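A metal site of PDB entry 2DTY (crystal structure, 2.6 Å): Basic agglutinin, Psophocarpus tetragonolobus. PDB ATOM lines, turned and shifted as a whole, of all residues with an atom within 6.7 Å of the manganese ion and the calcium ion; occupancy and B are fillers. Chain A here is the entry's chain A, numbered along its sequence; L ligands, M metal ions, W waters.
Within 4 Å of the manganese ion: Glu 122, Asp 124, Asp 131 and His 136. Along chain A the residues within 4 Å of the manganese ion span positions 122 to 136. The nearest printed residue that does not touch the manganese ion is Ser 146 (4.2 Å).
An oxygen (O3) of the ligand is in hydrogen-bond range of the side-chain amide nitrogen (ND2) of Asn 128 (3.1 Å). N of Gly 105 sits at hydrogen-bond distance from O3 of the ligand (2.7 Å). The side-chain carboxylate (OD2) of Asp 87 sits at hydrogen-bond distance from an oxygen (O3) of the ligand, at 2.6 Å.
The calcium ion is bound by OD2 of Asp 131 (2.3 Å), O of Phe 126 (2.4 Å), water W2 (2.4 Å), water W1 (2.5 Å), OD1 of Asp 124 (2.5 Å), OD1 of Asn 128 (2.5 Å) and OD2 of Asp 124 (2.6 Å). The calcium ion has seven donor atoms within binding distance.
Water W4 lies within hydrogen-bond range of O of Val 144 (2.8 Å), OE1 of Glu 122 (2.9 Å) and NE1 of Trp 130 (3.5 Å). Water W1 bridges the backbone carbonyl oxygen of Gly 105 and the indole nitrogen of Trp 130.
The backbone carbonyl oxygen (O) of Asp 131 lies within hydrogen-bond range of the guanidinium group (NE) of Arg 127 (3.2 Å). The side-chain carboxylate of Glu 122 sits at hydrogen-bond distance from the side-chain hydroxyl of Ser 146 (3.4 Å). The side-chain carboxylate (OE1) of Glu 122 lies close to the side-chain carboxylate (OD2) of Asp 140. N of Glu 122 is in hydrogen-bond range of O of Gly 138, 2.8 Å away.
The manganese ion is bound by the side-chain carboxylate of Asp 131, the side-chain carboxylate of Glu 122, the side-chain carboxylate of Asp 124, a ring nitrogen (NE2) of His 136, water W3 and water W4.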
ATOM      1  N   ASP A  87       4.670 -20.860  -2.277  1.00  0.00           N
ATOM      2  CA  ASP A  87       4.850 -19.459  -1.893  1.00  0.00           C
ATOM      3  C   ASP A  87       3.819 -18.555  -2.591  1.00  0.00           C
ATOM      4  O   ASP A  87       3.475 -17.474  -2.106  1.00  0.00           O
ATOM      5  CB  ASP A  87       6.250 -18.973  -2.281  1.00  0.00           C
ATOM      6  CG  ASP A  87       7.325 -19.358  -1.273  1.00  0.00           C
ATOM      7  OD1 ASP A  87       7.900 -20.464  -1.381  1.00  0.00           O
ATOM      8  OD2 ASP A  87       7.572 -18.540  -0.360  1.00  0.00           O
ATOM      9  N   GLY A 104      11.317 -19.853  -4.083  1.00  0.00           N
ATOM     10  CA  GLY A 104      10.824 -19.442  -2.790  1.00  0.00           C
ATOM     11  C   GLY A 104      10.088 -18.127  -2.830  1.00  0.00           C
ATOM     12  O   GLY A 104       9.298 -17.880  -3.734  1.00  0.00           O
ATOM     13  N   GLY A 105      10.359 -17.270  -1.842  1.00  0.00           N
ATOM     14  CA  GLY A 105       9.709 -15.984  -1.764  1.00  0.00           C
ATOM     15  C   GLY A 105       9.915 -15.083  -2.960  1.00  0.00           C
ATOM     16  O   GLY A 105       9.258 -14.056  -3.087  1.00  0.00           O
ATOM     17  N   TYR A 106      10.834 -15.454  -3.856  1.00  0.00           N
ATOM     18  CA  TYR A 106      11.093 -14.642  -5.031  1.00  0.00           C
ATOM     19  C   TYR A 106      10.294 -15.087  -6.267  1.00  0.00           C
ATOM     20  O   TYR A 106      10.443 -14.505  -7.359  1.00  0.00           O
ATOM     21  CB  TYR A 106      12.595 -14.605  -5.307  1.00  0.00           C
ATOM     22  CG  TYR A 106      13.367 -13.883  -4.204  1.00  0.00           C
ATOM     23  CD1 TYR A 106      13.094 -12.550  -3.896  1.00  0.00           C
ATOM     24  CD2 TYR A 106      14.327 -14.543  -3.443  1.00  0.00           C
ATOM     25  CE1 TYR A 106      13.767 -11.889  -2.874  1.00  0.00           C
ATOM     26  CE2 TYR A 106      15.008 -13.891  -2.412  1.00  0.00           C
ATOM     27  CZ  TYR A 106      14.718 -12.562  -2.129  1.00  0.00           C
ATOM     28  OH  TYR A 106      15.379 -11.913  -1.108  1.00  0.00           O
ATOM     29  N   PHE A 107       9.442 -16.093  -6.083  1.00  0.00           N
ATOM     30  CA  PHE A 107       8.554 -16.599  -7.139  1.00  0.00           C
ATOM     31  C   PHE A 107       9.218 -17.013  -8.457  1.00  0.00           C
ATOM     32  O   PHE A 107       8.530 -17.347  -9.417  1.00  0.00           O
ATOM     33  CB  PHE A 107       7.499 -15.544  -7.474  1.00  0.00           C
ATOM     34  CG  PHE A 107       6.780 -14.999  -6.280  1.00  0.00           C
ATOM     35  CD1 PHE A 107       5.911 -15.788  -5.555  1.00  0.00           C
ATOM     36  CD2 PHE A 107       6.924 -13.663  -5.929  1.00  0.00           C
ATOM     37  CE1 PHE A 107       5.180 -15.256  -4.464  1.00  0.00           C
ATOM     38  CE2 PHE A 107       6.208 -13.126  -4.858  1.00  0.00           C
ATOM     39  CZ  PHE A 107       5.336 -13.923  -4.125  1.00  0.00           C
ATOM     40  N   GLU A 122       1.296 -10.115  -7.904  1.00  0.00           N
ATOM     41  CA  GLU A 122       1.469 -11.335  -7.140  1.00  0.00           C
ATOM     42  C   GLU A 122       0.271 -11.754  -6.299  1.00  0.00           C
ATOM     43  O   GLU A 122      -0.548 -10.944  -5.864  1.00  0.00           O
ATOM     44  CB  GLU A 122       2.665 -11.196  -6.204  1.00  0.00           C
ATOM     45  CG  GLU A 122       2.389 -10.222  -5.067  1.00  0.00           C
ATOM     46  CD  GLU A 122       3.454 -10.244  -3.990  1.00  0.00           C
ATOM     47  OE1 GLU A 122       4.615  -9.872  -4.274  1.00  0.00           O
ATOM     48  OE2 GLU A 122       3.138 -10.622  -2.852  1.00  0.00           O
ATOM     49  N   ASP A 124       0.428 -13.792  -3.189  1.00  0.00           N
ATOM     50  CA  ASP A 124       1.332 -14.288  -2.151  1.00  0.00           C
ATOM     51  C   ASP A 124       0.664 -15.090  -1.048  1.00  0.00           C
ATOM     52  O   ASP A 124      -0.211 -14.592  -0.358  1.00  0.00           O
ATOM     53  CB  ASP A 124       2.056 -13.101  -1.524  1.00  0.00           C
ATOM     54  CG  ASP A 124       3.416 -13.463  -0.989  1.00  0.00           C
ATOM     55  OD1 ASP A 124       3.641 -14.652  -0.663  1.00  0.00           O
ATOM     56  OD2 ASP A 124       4.268 -12.555  -0.894  1.00  0.00           O
ATOM     57  N   THR A 125       1.120 -16.324  -0.878  1.00  0.00           N
ATOM     58  CA  THR A 125       0.557 -17.211   0.141  1.00  0.00           C
ATOM     59  C   THR A 125       1.444 -17.414   1.379  1.00  0.00           C
ATOM     60  O   THR A 125       0.972 -17.923   2.392  1.00  0.00           O
ATOM     61  CB  THR A 125       0.217 -18.570  -0.491  1.00  0.00           C
ATOM     62  OG1 THR A 125       1.368 -19.076  -1.171  1.00  0.00           O
ATOM     63  CG2 THR A 125      -0.929 -18.402  -1.503  1.00  0.00           C
ATOM     64  N   PHE A 126       2.713 -17.031   1.288  1.00  0.00           N
ATOM     65  CA  PHE A 126       3.646 -17.173   2.403  1.00  0.00           C
ATOM     66  C   PHE A 126       4.154 -15.817   2.866  1.00  0.00           C
ATOM     67  O   PHE A 126       4.475 -14.942   2.060  1.00  0.00           O
ATOM     68  CB  PHE A 126       4.838 -18.015   1.990  1.00  0.00           C
ATOM     69  CG  PHE A 126       5.844 -18.185   3.077  1.00  0.00           C
ATOM     70  CD1 PHE A 126       5.647 -19.125   4.082  1.00  0.00           C
ATOM     71  CD2 PHE A 126       6.974 -17.372   3.142  1.00  0.00           C
ATOM     72  CE1 PHE A 126       6.555 -19.248   5.133  1.00  0.00           C
ATOM     73  CE2 PHE A 126       7.887 -17.489   4.172  1.00  0.00           C
ATOM     74  CZ  PHE A 126       7.680 -18.427   5.175  1.00  0.00           C
ATOM     75  N   ARG A 127       4.245 -15.644   4.180  1.00  0.00           N
ATOM     76  CA  ARG A 127       4.707 -14.379   4.739  1.00  0.00           C
ATOM     77  C   ARG A 127       6.214 -14.304   4.988  1.00  0.00           C
ATOM     78  O   ARG A 127       6.706 -14.839   5.978  1.00  0.00           O
ATOM     79  CB  ARG A 127       3.952 -14.085   6.037  1.00  0.00           C
ATOM     80  CG  ARG A 127       4.186 -12.679   6.575  1.00  0.00           C
ATOM     81  CD  ARG A 127       3.229 -12.320   7.703  1.00  0.00           C
ATOM     82  NE  ARG A 127       3.411 -10.926   8.123  1.00  0.00           N
ATOM     83  CZ  ARG A 127       2.726 -10.331   9.090  1.00  0.00           C
ATOM     84  NH1 ARG A 127       1.795 -11.002   9.763  1.00  0.00           N
ATOM     85  NH2 ARG A 127       2.952  -9.062   9.381  1.00  0.00           N
ATOM     86  N   ASN A 128       6.940 -13.633   4.096  1.00  0.00           N
ATOM     87  CA  ASN A 128       8.368 -13.456   4.268  1.00  0.00           C
ATOM     88  C   ASN A 128       8.619 -12.273   5.187  1.00  0.00           C
ATOM     89  O   ASN A 128       7.690 -11.580   5.598  1.00  0.00           O
ATOM     90  CB  ASN A 128       9.065 -13.194   2.934  1.00  0.00           C
ATOM     91  CG  ASN A 128       9.111 -14.411   2.053  1.00  0.00           C
ATOM     92  OD1 ASN A 128       8.138 -14.711   1.360  1.00  0.00           O
ATOM     93  ND2 ASN A 128      10.224 -15.141   2.088  1.00  0.00           N
ATOM     94  N   TRP A 130       9.609  -9.455   4.576  1.00  0.00           N
ATOM     95  CA  TRP A 130       9.174  -8.200   3.962  1.00  0.00           C
ATOM     96  C   TRP A 130       7.691  -8.138   3.611  1.00  0.00           C
ATOM     97  O   TRP A 130       7.248  -7.177   2.972  1.00  0.00           O
ATOM     98  CB  TRP A 130       9.989  -7.966   2.688  1.00  0.00           C
ATOM     99  CG  TRP A 130       9.817  -9.086   1.688  1.00  0.00           C
ATOM    100  CD1 TRP A 130       8.724  -9.344   0.907  1.00  0.00           C
ATOM    101  CD2 TRP A 130      10.760 -10.133   1.403  1.00  0.00           C
ATOM    102  NE1 TRP A 130       8.924 -10.480   0.159  1.00  0.00           N
ATOM    103  CE2 TRP A 130      10.161 -10.994   0.447  1.00  0.00           C
ATOM    104  CE3 TRP A 130      12.052 -10.439   1.865  1.00  0.00           C
ATOM    105  CZ2 TRP A 130      10.811 -12.125  -0.057  1.00  0.00           C
ATOM    106  CZ3 TRP A 130      12.701 -11.578   1.355  1.00  0.00           C
ATOM    107  CH2 TRP A 130      12.076 -12.405   0.407  1.00  0.00           C
ATOM    108  N   ASP A 131       6.926  -9.151   4.020  1.00  0.00           N
ATOM    109  CA  ASP A 131       5.490  -9.240   3.713  1.00  0.00           C
ATOM    110  C   ASP A 131       4.550  -8.906   4.837  1.00  0.00           C
ATOM    111  O   ASP A 131       4.895  -9.025   6.011  1.00  0.00           O
ATOM    112  CB  ASP A 131       5.094 -10.666   3.296  1.00  0.00           C
ATOM    113  CG  ASP A 131       5.495 -11.025   1.890  1.00  0.00           C
ATOM    114  OD1 ASP A 131       5.374 -10.169   1.000  1.00  0.00           O
ATOM    115  OD2 ASP A 131       5.917 -12.184   1.675  1.00  0.00           O
ATOM    116  N   PRO A 132       3.333  -8.468   4.484  1.00  0.00           N
ATOM    117  CA  PRO A 132       2.291  -8.131   5.445  1.00  0.00           C
ATOM    118  C   PRO A 132       1.490  -9.428   5.571  1.00  0.00           C
ATOM    119  O   PRO A 132       1.850 -10.420   4.934  1.00  0.00           O
ATOM    120  CB  PRO A 132       1.514  -7.037   4.736  1.00  0.00           C
ATOM    121  CG  PRO A 132       1.582  -7.464   3.327  1.00  0.00           C
ATOM    122  CD  PRO A 132       3.044  -7.843   3.184  1.00  0.00           C
ATOM    123  N   ILE A 134      -0.708 -12.614   5.095  1.00  0.00           N
ATOM    124  CA  ILE A 134      -1.026 -13.327   3.855  1.00  0.00           C
ATOM    125  C   ILE A 134      -2.337 -14.083   4.019  1.00  0.00           C
ATOM    126  O   ILE A 134      -2.790 -14.336   5.125  1.00  0.00           O
ATOM    127  CB  ILE A 134       0.100 -14.337   3.459  1.00  0.00           C
ATOM    128  CG1 ILE A 134       0.474 -15.259   4.637  1.00  0.00           C
ATOM    129  CG2 ILE A 134       1.334 -13.569   3.020  1.00  0.00           C
ATOM    130  CD1 ILE A 134      -0.545 -16.348   4.951  1.00  0.00           C
ATOM    131  N   HIS A 136      -2.220 -12.203   0.119  1.00  0.00           N
ATOM    132  CA  HIS A 136      -2.453 -10.848  -0.324  1.00  0.00           C
ATOM    133  C   HIS A 136      -2.106 -10.665  -1.793  1.00  0.00           C
ATOM    134  O   HIS A 136      -1.289 -11.389  -2.347  1.00  0.00           O
ATOM    135  CB  HIS A 136      -1.664  -9.843   0.540  1.00  0.00           C
ATOM    136  CG  HIS A 136      -0.185 -10.066   0.552  1.00  0.00           C
ATOM    137  ND1 HIS A 136       0.488 -10.577   1.647  1.00  0.00           N
ATOM    138  CD2 HIS A 136       0.770  -9.833  -0.386  1.00  0.00           C
ATOM    139  CE1 HIS A 136       1.782 -10.631   1.392  1.00  0.00           C
ATOM    140  NE2 HIS A 136       1.982 -10.196   0.165  1.00  0.00           N
ATOM    141  N   ILE A 137      -2.767  -9.700  -2.423  1.00  0.00           N
ATOM    142  CA  ILE A 137      -2.512  -9.363  -3.809  1.00  0.00           C
ATOM    143  C   ILE A 137      -1.480  -8.273  -3.673  1.00  0.00           C
ATOM    144  O   ILE A 137      -1.520  -7.502  -2.713  1.00  0.00           O
ATOM    145  CB  ILE A 137      -3.736  -8.747  -4.481  1.00  0.00           C
ATOM    146  CG1 ILE A 137      -4.927  -9.698  -4.372  1.00  0.00           C
ATOM    147  CG2 ILE A 137      -3.437  -8.462  -5.928  1.00  0.00           C
ATOM    148  CD1 ILE A 137      -6.197  -9.152  -4.984  1.00  0.00           C
ATOM    149  N   GLY A 138      -0.543  -8.195  -4.607  1.00  0.00           N
ATOM    150  CA  GLY A 138       0.455  -7.156  -4.505  1.00  0.00           C
ATOM    151  C   GLY A 138       0.965  -6.751  -5.859  1.00  0.00           C
ATOM    152  O   GLY A 138       1.043  -7.564  -6.788  1.00  0.00           O
ATOM    153  N   ASP A 140       4.123  -5.452  -7.775  1.00  0.00           N
ATOM    154  CA  ASP A 140       5.566  -5.365  -7.655  1.00  0.00           C
ATOM    155  C   ASP A 140       6.226  -4.714  -8.861  1.00  0.00           C
ATOM    156  O   ASP A 140       5.910  -5.032 -10.010  1.00  0.00           O
ATOM    157  CB  ASP A 140       6.171  -6.756  -7.449  1.00  0.00           C
ATOM    158  CG  ASP A 140       5.509  -7.515  -6.332  1.00  0.00           C
ATOM    159  OD1 ASP A 140       4.966  -6.875  -5.412  1.00  0.00           O
ATOM    160  OD2 ASP A 140       5.526  -8.763  -6.368  1.00  0.00           O
ATOM    161  N   VAL A 144      10.276  -7.682  -5.138  1.00  0.00           N
ATOM    162  CA  VAL A 144       9.210  -8.501  -4.600  1.00  0.00           C
ATOM    163  C   VAL A 144       8.611  -7.834  -3.375  1.00  0.00           C
ATOM    164  O   VAL A 144       7.719  -8.383  -2.729  1.00  0.00           O
ATOM    165  CB  VAL A 144       9.726  -9.895  -4.260  1.00  0.00           C
ATOM    166  CG1 VAL A 144      10.532  -9.861  -2.969  1.00  0.00           C
ATOM    167  CG2 VAL A 144       8.570 -10.860  -4.180  1.00  0.00           C
ATOM    168  N   ILE A 145       9.112  -6.651  -3.035  1.00  0.00           N
ATOM    169  CA  ILE A 145       8.571  -5.923  -1.888  1.00  0.00           C
ATOM    170  C   ILE A 145       7.580  -4.903  -2.475  1.00  0.00           C
ATOM    171  O   ILE A 145       7.943  -3.794  -2.858  1.00  0.00           O
ATOM    172  CB  ILE A 145       9.691  -5.224  -1.092  1.00  0.00           C
ATOM    173  CG1 ILE A 145       9.092  -4.414   0.055  1.00  0.00           C
ATOM    174  CG2 ILE A 145      10.498  -4.324  -1.978  1.00  0.00           C
ATOM    175  CD1 ILE A 145      10.128  -3.706   0.914  1.00  0.00           C
ATOM    176  N   SER A 146       6.323  -5.340  -2.546  1.00  0.00           N
ATOM    177  CA  SER A 146       5.198  -4.598  -3.132  1.00  0.00           C
ATOM    178  C   SER A 146       5.021  -3.132  -2.819  1.00  0.00           C
ATOM    179  O   SER A 146       5.298  -2.685  -1.719  1.00  0.00           O
ATOM    180  CB  SER A 146       3.896  -5.318  -2.773  1.00  0.00           C
ATOM    181  OG  SER A 146       3.997  -6.698  -3.090  1.00  0.00           O
ATOM    182  N   THR A 149      -0.547  -3.264  -1.465  1.00  0.00           N
ATOM    183  CA  THR A 149      -0.955  -4.594  -1.053  1.00  0.00           C
ATOM    184  C   THR A 149      -2.381  -4.628  -0.532  1.00  0.00           C
ATOM    185  O   THR A 149      -2.850  -3.667   0.050  1.00  0.00           O
ATOM    186  CB  THR A 149       0.000  -5.128   0.054  1.00  0.00           C
ATOM    187  OG1 THR A 149       1.155  -5.706  -0.550  1.00  0.00           O
ATOM    188  CG2 THR A 149      -0.680  -6.146   0.920  1.00  0.00           C
HETATM  189  O1  LIG L   1      11.305 -21.020   3.165  1.00  0.00           O
HETATM  190  C1  LIG L   1      12.129 -19.770   3.145  1.00  0.00           C
HETATM  191  O2  LIG L   1      11.971 -18.990   4.342  1.00  0.00           O
HETATM  192  C2  LIG L   1      11.729 -18.916   1.879  1.00  0.00           C
HETATM  193  N1  LIG L   1      12.499 -17.677   1.857  1.00  0.00           N
HETATM  194  C3  LIG L   1      10.179 -18.636   1.908  1.00  0.00           C
HETATM  195  O3  LIG L   1       9.811 -17.866   0.774  1.00  0.00           O
HETATM  196  C4  LIG L   1       9.413 -19.976   1.921  1.00  0.00           C
HETATM  197  O4  LIG L   1       9.674 -20.710   0.721  1.00  0.00           O
HETATM  198  C5  LIG L   1       9.845 -20.793   3.164  1.00  0.00           C
HETATM  199  C6  LIG L   1       9.141 -22.144   3.218  1.00  0.00           C
HETATM  200  O5  LIG L   1       9.285 -22.822   4.471  1.00  0.00           O
HETATM  201  C7  LIG L   1      13.079 -17.204   0.736  1.00  0.00           C
HETATM  202  O6  LIG L   1      13.022 -17.756  -0.367  1.00  0.00           O
HETATM  203  C8  LIG L   1      13.839 -15.891   0.882  1.00  0.00           C
HETATM  204 MN    MN M   1       4.102 -10.230  -0.833  1.00  0.00          MN
HETATM  205 CA    CA M   2       5.891 -14.117   0.342  1.00  0.00          CA
HETATM  206  O   HOH W   1       7.397 -13.065  -1.311  1.00  0.00           O
HETATM  207  O   HOH W   2       6.286 -16.114  -0.979  1.00  0.00           O
HETATM  208  O   HOH W   3       4.425  -7.901  -0.729  1.00  0.00           O
HETATM  209  O   HOH W   4       6.245 -10.614  -2.013  1.00  0.00           O
